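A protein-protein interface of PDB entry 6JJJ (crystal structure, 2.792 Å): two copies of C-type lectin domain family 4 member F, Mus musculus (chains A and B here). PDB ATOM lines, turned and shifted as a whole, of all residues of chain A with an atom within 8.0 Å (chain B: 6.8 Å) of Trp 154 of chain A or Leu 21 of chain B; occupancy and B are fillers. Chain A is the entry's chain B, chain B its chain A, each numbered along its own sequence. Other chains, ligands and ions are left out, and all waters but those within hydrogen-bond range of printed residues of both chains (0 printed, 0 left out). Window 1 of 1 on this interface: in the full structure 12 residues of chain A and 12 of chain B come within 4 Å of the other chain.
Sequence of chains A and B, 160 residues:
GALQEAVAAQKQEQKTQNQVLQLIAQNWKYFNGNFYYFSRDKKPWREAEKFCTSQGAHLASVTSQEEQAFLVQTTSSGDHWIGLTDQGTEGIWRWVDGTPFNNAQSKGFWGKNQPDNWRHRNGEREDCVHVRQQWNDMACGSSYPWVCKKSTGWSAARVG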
ATOM      1  N   GLU A  13      20.789  19.217 -31.807  1.00  0.00           N
ATOM      2  CA  GLU A  13      20.023  17.981 -31.690  1.00  0.00           C
ATOM      3  C   GLU A  13      20.649  17.063 -30.652  1.00  0.00           C
ATOM      4  O   GLU A  13      19.940  16.455 -29.838  1.00  0.00           O
ATOM      5  CB  GLU A  13      19.948  17.283 -33.047  1.00  0.00           C
ATOM      6  CG  GLU A  13      19.036  16.067 -33.083  1.00  0.00           C
ATOM      7  CD  GLU A  13      17.564  16.437 -32.991  1.00  0.00           C
ATOM      8  OE1 GLU A  13      17.206  17.564 -33.391  1.00  0.00           O
ATOM      9  OE2 GLU A  13      16.765  15.599 -32.521  1.00  0.00           O
ATOM     10  N   GLN A  14      21.980  16.956 -30.658  1.00  0.00           N
ATOM     11  CA  GLN A  14      22.662  16.136 -29.663  1.00  0.00           C
ATOM     12  C   GLN A  14      22.284  16.552 -28.247  1.00  0.00           C
ATOM     13  O   GLN A  14      22.208  15.713 -27.341  1.00  0.00           O
ATOM     14  CB  GLN A  14      24.174  16.212 -29.878  1.00  0.00           C
ATOM     15  CG  GLN A  14      24.955  15.019 -29.357  1.00  0.00           C
ATOM     16  CD  GLN A  14      25.394  14.093 -30.482  1.00  0.00           C
ATOM     17  OE1 GLN A  14      26.580  14.009 -30.803  1.00  0.00           O
ATOM     18  NE2 GLN A  14      24.435  13.403 -31.095  1.00  0.00           N
ATOM     19  N   THR A  16      19.318  18.043 -27.174  1.00  0.00           N
ATOM     20  CA  THR A  16      17.986  17.497 -26.931  1.00  0.00           C
ATOM     21  C   THR A  16      18.021  15.972 -26.871  1.00  0.00           C
ATOM     22  O   THR A  16      17.484  15.364 -25.939  1.00  0.00           O
ATOM     23  CB  THR A  16      17.019  17.984 -28.010  1.00  0.00           C
ATOM     24  OG1 THR A  16      17.458  17.476 -29.273  1.00  0.00           O
ATOM     25  CG2 THR A  16      17.022  19.510 -28.047  1.00  0.00           C
ATOM     26  N   GLN A  17      18.633  15.338 -27.875  1.00  0.00           N
ATOM     27  CA  GLN A  17      18.775  13.886 -27.888  1.00  0.00           C
ATOM     28  C   GLN A  17      19.309  13.377 -26.558  1.00  0.00           C
ATOM     29  O   GLN A  17      18.941  12.283 -26.118  1.00  0.00           O
ATOM     30  CB  GLN A  17      19.694  13.495 -29.047  1.00  0.00           C
ATOM     31  CG  GLN A  17      19.573  12.064 -29.530  1.00  0.00           C
ATOM     32  CD  GLN A  17      20.302  11.840 -30.848  1.00  0.00           C
ATOM     33  OE1 GLN A  17      21.482  12.173 -30.988  1.00  0.00           O
ATOM     34  NE2 GLN A  17      19.593  11.291 -31.829  1.00  0.00           N
ATOM     35  N   ASN A  18      20.171  14.155 -25.899  1.00  0.00           N
ATOM     36  CA  ASN A  18      20.655  13.772 -24.579  1.00  0.00           C
ATOM     37  C   ASN A  18      19.586  13.997 -23.515  1.00  0.00           C
ATOM     38  O   ASN A  18      19.411  13.164 -22.618  1.00  0.00           O
ATOM     39  CB  ASN A  18      21.920  14.560 -24.238  1.00  0.00           C
ATOM     40  CG  ASN A  18      22.534  14.140 -22.916  1.00  0.00           C
ATOM     41  OD1 ASN A  18      22.004  13.278 -22.216  1.00  0.00           O
ATOM     42  ND2 ASN A  18      23.660  14.753 -22.567  1.00  0.00           N
ATOM     43  N   GLN A  19      18.854  15.112 -23.605  1.00  0.00           N
ATOM     44  CA  GLN A  19      17.871  15.439 -22.577  1.00  0.00           C
ATOM     45  C   GLN A  19      16.857  14.316 -22.401  1.00  0.00           C
ATOM     46  O   GLN A  19      16.437  14.017 -21.278  1.00  0.00           O
ATOM     47  CB  GLN A  19      17.159  16.746 -22.931  1.00  0.00           C
ATOM     48  CG  GLN A  19      16.137  17.209 -21.901  1.00  0.00           C
ATOM     49  CD  GLN A  19      15.552  18.570 -22.232  1.00  0.00           C
ATOM     50  OE1 GLN A  19      16.050  19.271 -23.110  1.00  0.00           O
ATOM     51  NE2 GLN A  19      14.488  18.947 -21.533  1.00  0.00           N
ATOM     52  N   VAL A  20      16.446  13.686 -23.503  1.00  0.00           N
ATOM     53  CA  VAL A  20      15.444  12.631 -23.418  1.00  0.00           C
ATOM     54  C   VAL A  20      16.052  11.355 -22.850  1.00  0.00           C
ATOM     55  O   VAL A  20      15.357  10.567 -22.197  1.00  0.00           O
ATOM     56  CB  VAL A  20      14.802  12.402 -24.798  1.00  0.00           C
ATOM     57  CG1 VAL A  20      14.257  13.714 -25.353  1.00  0.00           C
ATOM     58  CG2 VAL A  20      15.807  11.794 -25.758  1.00  0.00           C
ATOM     59  N   LEU A  21      17.346  11.120 -23.095  1.00  0.00           N
ATOM     60  CA  LEU A  21      18.016   9.976 -22.483  1.00  0.00           C
ATOM     61  C   LEU A  21      17.952  10.060 -20.964  1.00  0.00           C
ATOM     62  O   LEU A  21      17.633   9.077 -20.286  1.00  0.00           O
ATOM     63  CB  LEU A  21      19.470   9.913 -22.943  1.00  0.00           C
ATOM     64  CG  LEU A  21      19.760   9.494 -24.378  1.00  0.00           C
ATOM     65  CD1 LEU A  21      21.225   9.766 -24.692  1.00  0.00           C
ATOM     66  CD2 LEU A  21      19.453   8.032 -24.599  1.00  0.00           C
ATOM     67  N   GLN A  22      18.268  11.233 -20.411  1.00  0.00           N
ATOM     68  CA  GLN A  22      18.195  11.420 -18.967  1.00  0.00           C
ATOM     69  C   GLN A  22      16.799  11.104 -18.451  1.00  0.00           C
ATOM     70  O   GLN A  22      16.643  10.526 -17.368  1.00  0.00           O
ATOM     71  CB  GLN A  22      18.595  12.857 -18.617  1.00  0.00           C
ATOM     72  CG  GLN A  22      20.037  13.204 -18.997  1.00  0.00           C
ATOM     73  CD  GLN A  22      20.339  14.696 -18.942  1.00  0.00           C
ATOM     74  OE1 GLN A  22      19.483  15.508 -18.594  1.00  0.00           O
ATOM     75  NE2 GLN A  22      21.566  15.061 -19.298  1.00  0.00           N
ATOM     76  N   LEU A  23      15.770  11.448 -19.226  1.00  0.00           N
ATOM     77  CA  LEU A  23      14.397  11.208 -18.797  1.00  0.00           C
ATOM     78  C   LEU A  23      14.074   9.718 -18.778  1.00  0.00           C
ATOM     79  O   LEU A  23      13.757   9.154 -17.725  1.00  0.00           O
ATOM     80  CB  LEU A  23      13.429  11.958 -19.712  1.00  0.00           C
ATOM     81  CG  LEU A  23      13.383  13.480 -19.581  1.00  0.00           C
ATOM     82  CD1 LEU A  23      12.553  14.091 -20.699  1.00  0.00           C
ATOM     83  CD2 LEU A  23      12.830  13.872 -18.214  1.00  0.00           C
ATOM     84  N   ILE A  24      14.150   9.056 -19.937  1.00  0.00           N
ATOM     85  CA  ILE A  24      13.777   7.647 -19.978  1.00  0.00           C
ATOM     86  C   ILE A  24      14.736   6.807 -19.146  1.00  0.00           C
ATOM     87  O   ILE A  24      14.346   5.762 -18.613  1.00  0.00           O
ATOM     88  CB  ILE A  24      13.699   7.147 -21.430  1.00  0.00           C
ATOM     89  CG1 ILE A  24      13.212   5.694 -21.475  1.00  0.00           C
ATOM     90  CG2 ILE A  24      15.057   7.246 -22.103  1.00  0.00           C
ATOM     91  CD1 ILE A  24      11.846   5.452 -20.842  1.00  0.00           C
ATOM     92  N   ALA A  25      15.991   7.237 -19.006  1.00  0.00           N
ATOM     93  CA  ALA A  25      16.908   6.526 -18.121  1.00  0.00           C
ATOM     94  C   ALA A  25      16.432   6.554 -16.676  1.00  0.00           C
ATOM     95  O   ALA A  25      16.818   5.681 -15.892  1.00  0.00           O
ATOM     96  CB  ALA A  25      18.314   7.120 -18.214  1.00  0.00           C
ATOM     97  N   TYR A  30       6.987   8.299 -22.352  1.00  0.00           N
ATOM     98  CA  TYR A  30       6.498   9.228 -23.356  1.00  0.00           C
ATOM     99  C   TYR A  30       5.070   8.876 -23.742  1.00  0.00           C
ATOM    100  O   TYR A  30       4.698   7.701 -23.797  1.00  0.00           O
ATOM    101  CB  TYR A  30       7.394   9.191 -24.598  1.00  0.00           C
ATOM    102  CG  TYR A  30       6.884  10.036 -25.744  1.00  0.00           C
ATOM    103  CD1 TYR A  30       5.962   9.529 -26.654  1.00  0.00           C
ATOM    104  CD2 TYR A  30       7.325  11.341 -25.916  1.00  0.00           C
ATOM    105  CE1 TYR A  30       5.489  10.300 -27.697  1.00  0.00           C
ATOM    106  CE2 TYR A  30       6.861  12.121 -26.959  1.00  0.00           C
ATOM    107  CZ  TYR A  30       5.946  11.596 -27.849  1.00  0.00           C
ATOM    108  OH  TYR A  30       5.484  12.377 -28.886  1.00  0.00           O
ATOM    109  N   PHE A  31       4.272   9.905 -24.013  1.00  0.00           N
ATOM    110  CA  PHE A  31       2.920   9.698 -24.518  1.00  0.00           C
ATOM    111  C   PHE A  31       2.442  10.986 -25.170  1.00  0.00           C
ATOM    112  O   PHE A  31       2.340  12.018 -24.497  1.00  0.00           O
ATOM    113  CB  PHE A  31       1.969   9.279 -23.403  1.00  0.00           C
ATOM    114  CG  PHE A  31       0.533   9.215 -23.836  1.00  0.00           C
ATOM    115  CD1 PHE A  31       0.022   8.069 -24.423  1.00  0.00           C
ATOM    116  CD2 PHE A  31      -0.301  10.307 -23.674  1.00  0.00           C
ATOM    117  CE1 PHE A  31      -1.297   8.011 -24.831  1.00  0.00           C
ATOM    118  CE2 PHE A  31      -1.618  10.257 -24.081  1.00  0.00           C
ATOM    119  CZ  PHE A  31      -2.118   9.108 -24.660  1.00  0.00           C
ATOM    120  N   ASN A  32       2.168  10.924 -26.468  1.00  0.00           N
ATOM    121  CA  ASN A  32       1.524  12.001 -27.218  1.00  0.00           C
ATOM    122  C   ASN A  32       2.067  13.373 -26.820  1.00  0.00           C
ATOM    123  O   ASN A  32       1.344  14.263 -26.368  1.00  0.00           O
ATOM    124  CB  ASN A  32       0.005  11.951 -27.045  1.00  0.00           C
ATOM    125  CG  ASN A  32      -0.667  11.010 -28.033  1.00  0.00           C
ATOM    126  OD1 ASN A  32      -0.134  10.740 -29.110  1.00  0.00           O
ATOM    127  ND2 ASN A  32      -1.845  10.514 -27.672  1.00  0.00           N
ATOM    128  N   GLY A  33       3.376  13.529 -26.997  1.00  0.00           N
ATOM    129  CA  GLY A  33       4.031  14.805 -26.869  1.00  0.00           C
ATOM    130  C   GLY A  33       4.654  15.069 -25.515  1.00  0.00           C
ATOM    131  O   GLY A  33       5.643  15.808 -25.433  1.00  0.00           O
ATOM    132  N   ASN A  34       4.114  14.479 -24.455  1.00  0.00           N
ATOM    133  CA  ASN A  34       4.577  14.762 -23.106  1.00  0.00           C
ATOM    134  C   ASN A  34       5.333  13.568 -22.541  1.00  0.00           C
ATOM    135  O   ASN A  34       5.205  12.436 -23.016  1.00  0.00           O
ATOM    136  CB  ASN A  34       3.405  15.111 -22.184  1.00  0.00           C
ATOM    137  CG  ASN A  34       2.552  16.236 -22.734  1.00  0.00           C
ATOM    138  OD1 ASN A  34       2.953  17.400 -22.720  1.00  0.00           O
ATOM    139  ND2 ASN A  34       1.361  15.893 -23.210  1.00  0.00           N
ATOM    140  N   PHE A  35       6.128  13.839 -21.509  1.00  0.00           N
ATOM    141  CA  PHE A  35       6.793  12.804 -20.730  1.00  0.00           C
ATOM    142  C   PHE A  35       6.116  12.691 -19.372  1.00  0.00           C
ATOM    143  O   PHE A  35       5.841  13.706 -18.722  1.00  0.00           O
ATOM    144  CB  PHE A  35       8.282  13.113 -20.563  1.00  0.00           C
ATOM    145  CG  PHE A  35       9.108  12.767 -21.767  1.00  0.00           C
ATOM    146  CD1 PHE A  35       9.548  11.469 -21.971  1.00  0.00           C
ATOM    147  CD2 PHE A  35       9.447  13.738 -22.693  1.00  0.00           C
ATOM    148  CE1 PHE A  35      10.309  11.147 -23.077  1.00  0.00           C
ATOM    149  CE2 PHE A  35      10.210  13.423 -23.804  1.00  0.00           C
ATOM    150  CZ  PHE A  35      10.641  12.127 -23.996  1.00  0.00           C
ATOM    151  N   SER A 151       6.473  18.728 -20.765  1.00  0.00           N
ATOM    152  CA  SER A 151       6.268  19.049 -22.168  1.00  0.00           C
ATOM    153  C   SER A 151       7.599  19.084 -22.909  1.00  0.00           C
ATOM    154  O   SER A 151       8.655  19.333 -22.321  1.00  0.00           O
ATOM    155  CB  SER A 151       5.550  20.392 -22.311  1.00  0.00           C
ATOM    156  OG  SER A 151       4.349  20.395 -21.559  1.00  0.00           O
ATOM    157  N   THR A 152       7.537  18.808 -24.210  1.00  0.00           N
ATOM    158  CA  THR A 152       8.713  18.854 -25.065  1.00  0.00           C
ATOM    159  C   THR A 152       8.278  19.156 -26.491  1.00  0.00           C
ATOM    160  O   THR A 152       7.120  18.948 -26.866  1.00  0.00           O
ATOM    161  CB  THR A 152       9.503  17.537 -25.037  1.00  0.00           C
ATOM    162  OG1 THR A 152       8.594  16.430 -24.996  1.00  0.00           O
ATOM    163  CG2 THR A 152      10.435  17.489 -23.833  1.00  0.00           C
ATOM    164  N   GLY A 153       9.224  19.653 -27.284  1.00  0.00           N
ATOM    165  CA  GLY A 153       9.017  19.799 -28.710  1.00  0.00           C
ATOM    166  C   GLY A 153       9.635  18.629 -29.446  1.00  0.00           C
ATOM    167  O   GLY A 153      10.172  18.774 -30.546  1.00  0.00           O
ATOM    168  N   TRP A 154       9.558  17.457 -28.822  1.00  0.00           N
ATOM    169  CA  TRP A 154      10.221  16.246 -29.285  1.00  0.00           C
ATOM    170  C   TRP A 154       9.186  15.163 -29.553  1.00  0.00           C
ATOM    171  O   TRP A 154       8.278  14.945 -28.744  1.00  0.00           O
ATOM    172  CB  TRP A 154      11.232  15.761 -28.241  1.00  0.00           C
ATOM    173  CG  TRP A 154      12.032  14.574 -28.664  1.00  0.00           C
ATOM    174  CD1 TRP A 154      13.214  14.585 -29.344  1.00  0.00           C
ATOM    175  CD2 TRP A 154      11.709  13.194 -28.442  1.00  0.00           C
ATOM    176  NE1 TRP A 154      13.651  13.301 -29.555  1.00  0.00           N
ATOM    177  CE2 TRP A 154      12.745  12.428 -29.013  1.00  0.00           C
ATOM    178  CE3 TRP A 154      10.647  12.535 -27.818  1.00  0.00           C
ATOM    179  CZ2 TRP A 154      12.748  11.035 -28.979  1.00  0.00           C
ATOM    180  CZ3 TRP A 154      10.654  11.152 -27.784  1.00  0.00           C
ATOM    181  CH2 TRP A 154      11.697  10.417 -28.361  1.00  0.00           C
ATOM    182  N   SER A 155       9.330  14.484 -30.687  1.00  0.00           N
ATOM    183  CA  SER A 155       8.405  13.420 -31.063  1.00  0.00           C
ATOM    184  C   SER A 155       9.100  12.351 -31.902  1.00  0.00           C
ATOM    185  O   SER A 155       9.904  12.660 -32.781  1.00  0.00           O
ATOM    186  CB  SER A 155       7.215  13.993 -31.837  1.00  0.00           C
ATOM    187  OG  SER A 155       7.638  14.598 -33.048  1.00  0.00           O
ATOM    188  N   GLN B  14      22.538   9.990 -36.189  1.00  0.00           N
ATOM    189  CA  GLN B  14      21.629  10.714 -35.309  1.00  0.00           C
ATOM    190  C   GLN B  14      20.178  10.363 -35.602  1.00  0.00           C
ATOM    191  O   GLN B  14      19.378  10.200 -34.671  1.00  0.00           O
ATOM    192  CB  GLN B  14      21.884  12.213 -35.458  1.00  0.00           C
ATOM    193  CG  GLN B  14      21.071  13.121 -34.555  1.00  0.00           C
ATOM    194  CD  GLN B  14      21.557  14.565 -34.602  1.00  0.00           C
ATOM    195  OE1 GLN B  14      21.050  15.385 -35.368  1.00  0.00           O
ATOM    196  NE2 GLN B  14      22.546  14.878 -33.776  1.00  0.00           N
ATOM    197  N   THR B  16      18.836   7.446 -36.918  1.00  0.00           N
ATOM    198  CA  THR B  16      18.546   6.152 -36.309  1.00  0.00           C
ATOM    199  C   THR B  16      18.555   6.278 -34.792  1.00  0.00           C
ATOM    200  O   THR B  16      17.608   5.865 -34.113  1.00  0.00           O
ATOM    201  CB  THR B  16      19.562   5.103 -36.761  1.00  0.00           C
ATOM    202  OG1 THR B  16      20.866   5.447 -36.276  1.00  0.00           O
ATOM    203  CG2 THR B  16      19.584   5.002 -38.266  1.00  0.00           C
ATOM    204  N   GLN B  17      19.559   6.905 -34.293  1.00  0.00           N
ATOM    205  CA  GLN B  17      19.558   7.071 -32.898  1.00  0.00           C
ATOM    206  C   GLN B  17      18.179   7.511 -32.496  1.00  0.00           C
ATOM    207  O   GLN B  17      17.507   6.903 -31.716  1.00  0.00           O
ATOM    208  CB  GLN B  17      20.522   8.154 -32.521  1.00  0.00           C
ATOM    209  CG  GLN B  17      21.885   7.652 -32.178  1.00  0.00           C
ATOM    210  CD  GLN B  17      22.616   8.615 -31.301  1.00  0.00           C
ATOM    211  OE1 GLN B  17      22.185   9.742 -31.104  1.00  0.00           O
ATOM    212  NE2 GLN B  17      23.725   8.178 -30.763  1.00  0.00           N
ATOM    213  N   ASN B  18      17.729   8.583 -33.070  1.00  0.00           N
ATOM    214  CA  ASN B  18      16.453   9.140 -32.634  1.00  0.00           C
ATOM    215  C   ASN B  18      15.348   8.093 -32.700  1.00  0.00           C
ATOM    216  O   ASN B  18      14.500   8.022 -31.804  1.00  0.00           O
ATOM    217  CB  ASN B  18      16.084  10.348 -33.494  1.00  0.00           C
ATOM    218  CG  ASN B  18      14.812  11.031 -33.021  1.00  0.00           C
ATOM    219  OD1 ASN B  18      14.684  11.387 -31.849  1.00  0.00           O
ATOM    220  ND2 ASN B  18      13.859  11.206 -33.931  1.00  0.00           N
ATOM    221  N   GLN B  19      15.342   7.274 -33.756  1.00  0.00           N
ATOM    222  CA  GLN B  19      14.275   6.295 -33.934  1.00  0.00           C
ATOM    223  C   GLN B  19      14.165   5.370 -32.728  1.00  0.00           C
ATOM    224  O   GLN B  19      13.057   5.008 -32.315  1.00  0.00           O
ATOM    225  CB  GLN B  19      14.519   5.485 -35.206  1.00  0.00           C
ATOM    226  CG  GLN B  19      13.435   4.468 -35.526  1.00  0.00           C
ATOM    227  CD  GLN B  19      13.663   3.786 -36.863  1.00  0.00           C
ATOM    228  OE1 GLN B  19      14.508   4.210 -37.650  1.00  0.00           O
ATOM    229  NE2 GLN B  19      12.908   2.724 -37.127  1.00  0.00           N
ATOM    230  N   VAL B  20      15.301   4.980 -32.151  1.00  0.00           N
ATOM    231  CA  VAL B  20      15.266   4.055 -31.027  1.00  0.00           C
ATOM    232  C   VAL B  20      14.777   4.763 -29.769  1.00  0.00           C
ATOM    233  O   VAL B  20      14.133   4.145 -28.912  1.00  0.00           O
ATOM    234  CB  VAL B  20      16.653   3.414 -30.828  1.00  0.00           C
ATOM    235  CG1 VAL B  20      17.142   2.790 -32.132  1.00  0.00           C
ATOM    236  CG2 VAL B  20      17.648   4.437 -30.314  1.00  0.00           C
ATOM    237  N   LEU B  21      15.055   6.063 -29.638  1.00  0.00           N
ATOM    238  CA  LEU B  21      14.530   6.818 -28.506  1.00  0.00           C
ATOM    239  C   LEU B  21      13.006   6.767 -28.481  1.00  0.00           C
ATOM    240  O   LEU B  21      12.399   6.494 -27.439  1.00  0.00           O
ATOM    241  CB  LEU B  21      15.008   8.266 -28.574  1.00  0.00           C
ATOM    242  CG  LEU B  21      16.478   8.536 -28.273  1.00  0.00           C
ATOM    243  CD1 LEU B  21      16.830   9.966 -28.654  1.00  0.00           C
ATOM    244  CD2 LEU B  21      16.785   8.304 -26.810  1.00  0.00           C
ATOM    245  N   GLN B  22      12.371   7.016 -29.629  1.00  0.00           N
ATOM    246  CA  GLN B  22      10.915   6.945 -29.701  1.00  0.00           C
ATOM    247  C   GLN B  22      10.417   5.575 -29.258  1.00  0.00           C
ATOM    248  O   GLN B  22       9.370   5.465 -28.609  1.00  0.00           O
ATOM    249  CB  GLN B  22      10.448   7.262 -31.123  1.00  0.00           C
ATOM    250  CG  GLN B  22      10.789   8.683 -31.582  1.00  0.00           C
ATOM    251  CD  GLN B  22      10.599   8.895 -33.079  1.00  0.00           C
ATOM    252  OE1 GLN B  22      10.189   7.987 -33.801  1.00  0.00           O
ATOM    253  NE2 GLN B  22      10.899  10.102 -33.547  1.00  0.00           N
ATOM    254  N   LEU B  23      11.170   4.521 -29.577  1.00  0.00           N
ATOM    255  CA  LEU B  23      10.766   3.169 -29.206  1.00  0.00           C
ATOM    256  C   LEU B  23      10.843   2.966 -27.698  1.00  0.00           C
ATOM    257  O   LEU B  23       9.836   2.662 -27.047  1.00  0.00           O
ATOM    258  CB  LEU B  23      11.644   2.150 -29.929  1.00  0.00           C
ATOM    259  CG  LEU B  23      11.436   2.005 -31.435  1.00  0.00           C
ATOM    260  CD1 LEU B  23      12.518   1.134 -32.049  1.00  0.00           C
ATOM    261  CD2 LEU B  23      10.049   1.430 -31.708  1.00  0.00           C
ATOM    262  N   ILE B  24      12.040   3.106 -27.123  1.00  0.00           N
ATOM    263  CA  ILE B  24      12.176   2.880 -25.690  1.00  0.00           C
ATOM    264  C   ILE B  24      11.399   3.930 -24.909  1.00  0.00           C
ATOM    265  O   ILE B  24      10.943   3.665 -23.790  1.00  0.00           O
ATOM    266  CB  ILE B  24      13.657   2.852 -25.275  1.00  0.00           C
ATOM    267  CG1 ILE B  24      13.791   2.516 -23.786  1.00  0.00           C
ATOM    268  CG2 ILE B  24      14.319   4.188 -25.573  1.00  0.00           C
ATOM    269  CD1 ILE B  24      13.179   1.177 -23.369  1.00  0.00           C
ATOM    270  N   ALA B  25      11.231   5.132 -25.468  1.00  0.00           N
ATOM    271  CA  ALA B  25      10.407   6.133 -24.799  1.00  0.00           C
ATOM    272  C   ALA B  25       8.959   5.674 -24.685  1.00  0.00           C
ATOM    273  O   ALA B  25       8.236   6.113 -23.784  1.00  0.00           O
ATOM    274  CB  ALA B  25      10.479   7.466 -25.542  1.00  0.00           C
ATOM    275  N   GLN B  26       8.521   4.789 -25.580  1.00  0.00           N
ATOM    276  CA  GLN B  26       7.192   4.197 -25.509  1.00  0.00           C
ATOM    277  C   GLN B  26       7.226   2.788 -24.930  1.00  0.00           C
ATOM    278  O   GLN B  26       6.260   2.034 -25.085  1.00  0.00           O
ATOM    279  CB  GLN B  26       6.544   4.205 -26.894  1.00  0.00           C
ATOM    280  CG  GLN B  26       6.448   5.598 -27.494  1.00  0.00           C
ATOM    281  CD  GLN B  26       5.828   5.608 -28.875  1.00  0.00           C
ATOM    282  OE1 GLN B  26       4.663   5.257 -29.048  1.00  0.00           O
ATOM    283  NE2 GLN B  26       6.610   6.007 -29.870  1.00  0.00           N
ATOM    284  N   ASN B  27       8.305   2.436 -24.232  1.00  0.00           N
ATOM    285  CA  ASN B  27       8.422   1.147 -23.550  1.00  0.00           C
ATOM    286  C   ASN B  27       8.493  -0.004 -24.559  1.00  0.00           C
ATOM    287  O   ASN B  27       7.781  -1.004 -24.447  1.00  0.00           O
ATOM    288  CB  ASN B  27       7.267   0.942 -22.563  1.00  0.00           C
ATOM    289  CG  ASN B  27       7.714   1.011 -21.110  1.00  0.00           C
ATOM    290  OD1 ASN B  27       8.863   0.716 -20.787  1.00  0.00           O
ATOM    291  ND2 ASN B  27       6.803   1.402 -20.228  1.00  0.00           N
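The side-chain amide nitrogen of Gln 17 of chain A is in hydrogen-bond range of the backbone carbonyl oxygen of Gln 14 of chain B, 3.1 Å away.
The side-chain amide oxygen (OE1) of Gln 17 of chain A sits close to the side-chain amide oxygen (OE1) of Gln 17 of chain B, at 2.5 Å.
The indole nitrogen of Trp 154 of chain A is in hydrogen-bond range of the side-chain amide oxygen of Asn 18 of chain B, 3.2 Å away.
The backbone carbonyl oxygen (O) of Ser 155 of chain A lies within hydrogen-bond range of the side-chain amide nitrogen (NE2) of Gln 22 of chain B, at 2.8 Å.
The backbone carbonyl oxygen (O) of Ala 25 of chain B lies within hydrogen-bond range of the backbone NH (N) of Tyr 30 of chain A.
The side-chain amide nitrogen of Asn 18 of chain B lies close to the side-chain amide nitrogen of Gln 22 of chain B, 3.2 Å away.
The side-chain amide nitrogen (NE2) of Gln 26 of chain B lies within hydrogen-bond range of the backbone carbonyl oxygen (O) of Gln 22 of chain B, at 3.1 Å.
OG1 of Thr 16 of chain A lies within hydrogen-bond range of O of Glu 13 of chain A, 2.7 Å away.
The side-chain amide nitrogen of Gln 14 of chain A lies within hydrogen-bond range of the side-chain amide oxygen of Gln 17 of chain A, at 3.2 Å.
OH of Tyr 30 of chain A lies within hydrogen-bond range of N of Gly 33 of chain A (3.1 Å).
CG of Glu 13 of chain A touches OE1 of Gln 14 of chain B, at 3.1 Å.
Gln 14 of chain A touches Gln 14 of chain B (NE2 to NE2, 3.6 Å).
Asn 18 of chain B touches Gln 17 of chain A (N to NE2, 3.5 Å).
Gln 17 of chain A touches Leu 21 of chain B.
CG2 of Val 20 of chain A touches CD1 of Leu 21 of chain B, at 3.6 Å.
Leu 21 of chain B touches Leu 21 of chain A (CD2 to CD2, 3.5 Å).
CD1 of Ile 24 of chain A touches O of Ile 24 of chain B, at 3.6 Å.
CB of Leu 21 of chain B touches CZ2 of Trp 154 of chain A (3.6 Å).
CH2 of Trp 154 of chain A touches N of Gln 22 of chain B, at 3.7 Å.
Printed residues of chain B within 4 Å of Glu 13 of chain A: Gln 14 (3.1 Å).
Of the printed residues of chain B, Gln 17 of chain A touches Gln 14 (3.1 Å), Gln 17 (2.5 Å), Asn 18 (3.5 Å) and Leu 21 (3.6 Å).
Leu 23 of chain A touches none of the printed residues of chain B.
Of the printed residues of chain B, Tyr 30 of chain A touches Ala 25 (2.9 Å).
No residue of chain B comes within 4 Å of Gly 153 of chain A.
Of chain B, only Asn 18, Leu 21 and Gln 22 come within 4 Å of Trp 154 of chain A.
Of the printed residues of chain A, Gln 14 of chain B touches Glu 13, Gln 14 and Gln 17.
Of the printed residues of chain A, Gln 17 of chain B touches Gln 17 (2.5 Å).
Leu 21 of chain B touches just these residues of chain A: Gln 17 (3.6 Å), Val 20 (3.6 Å), Leu 21 (3.5 Å) and Trp 154 (3.6 Å).
The nearest residue of chain A that does not touch Leu 21 of chain B is Ile 24 of chain A (5.1 Å).
The nearest printed residue of chain A that does not touch Ile 24 of chain B is Tyr 30 of chain A (6.3 Å).
Of the 23 printed residues of chain A, 9 touch a printed residue of chain B.
Printed residues of chain A that touch a printed residue of chain B: Glu 13, Gln 14, Gln 17, Val 20, Leu 21, Ile 24, Tyr 30, Trp 154 and Ser 155.
Printed residues of chain B that touch a printed residue of chain A: Gln 14, Gln 17, Asn 18, Leu 21, Gln 22, Ile 24 and Ala 25.
Hydrophobic or aromatic side chains of chain B that line the printed part of chain A: Leu 21, Ile 24 and Ala 25.
Among the printed residues, 14 pairs touch across the chains.
Among the printed residues, no Asp or Glu carboxylate lies within 4 Å of a Lys or Arg side-chain nitrogen of the other chain.
Gln 14 of chain A touches its own counterpart, Gln 14 of chain B.
Gln 17 of chain B touches its own counterpart, Gln 17 of chain A.
Gln 17 of chain A touches Leu 21 of chain B, but with the chains exchanged Leu 21 of chain A does not touch Gln 17 of chain B (6.5 Å).
Ile 24 of chain B touches its own counterpart, Ile 24 of chain A.
Of the 14 pairs that touch across the chains among the printed residues, 4 have their exchanged pair printed and touching as well.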
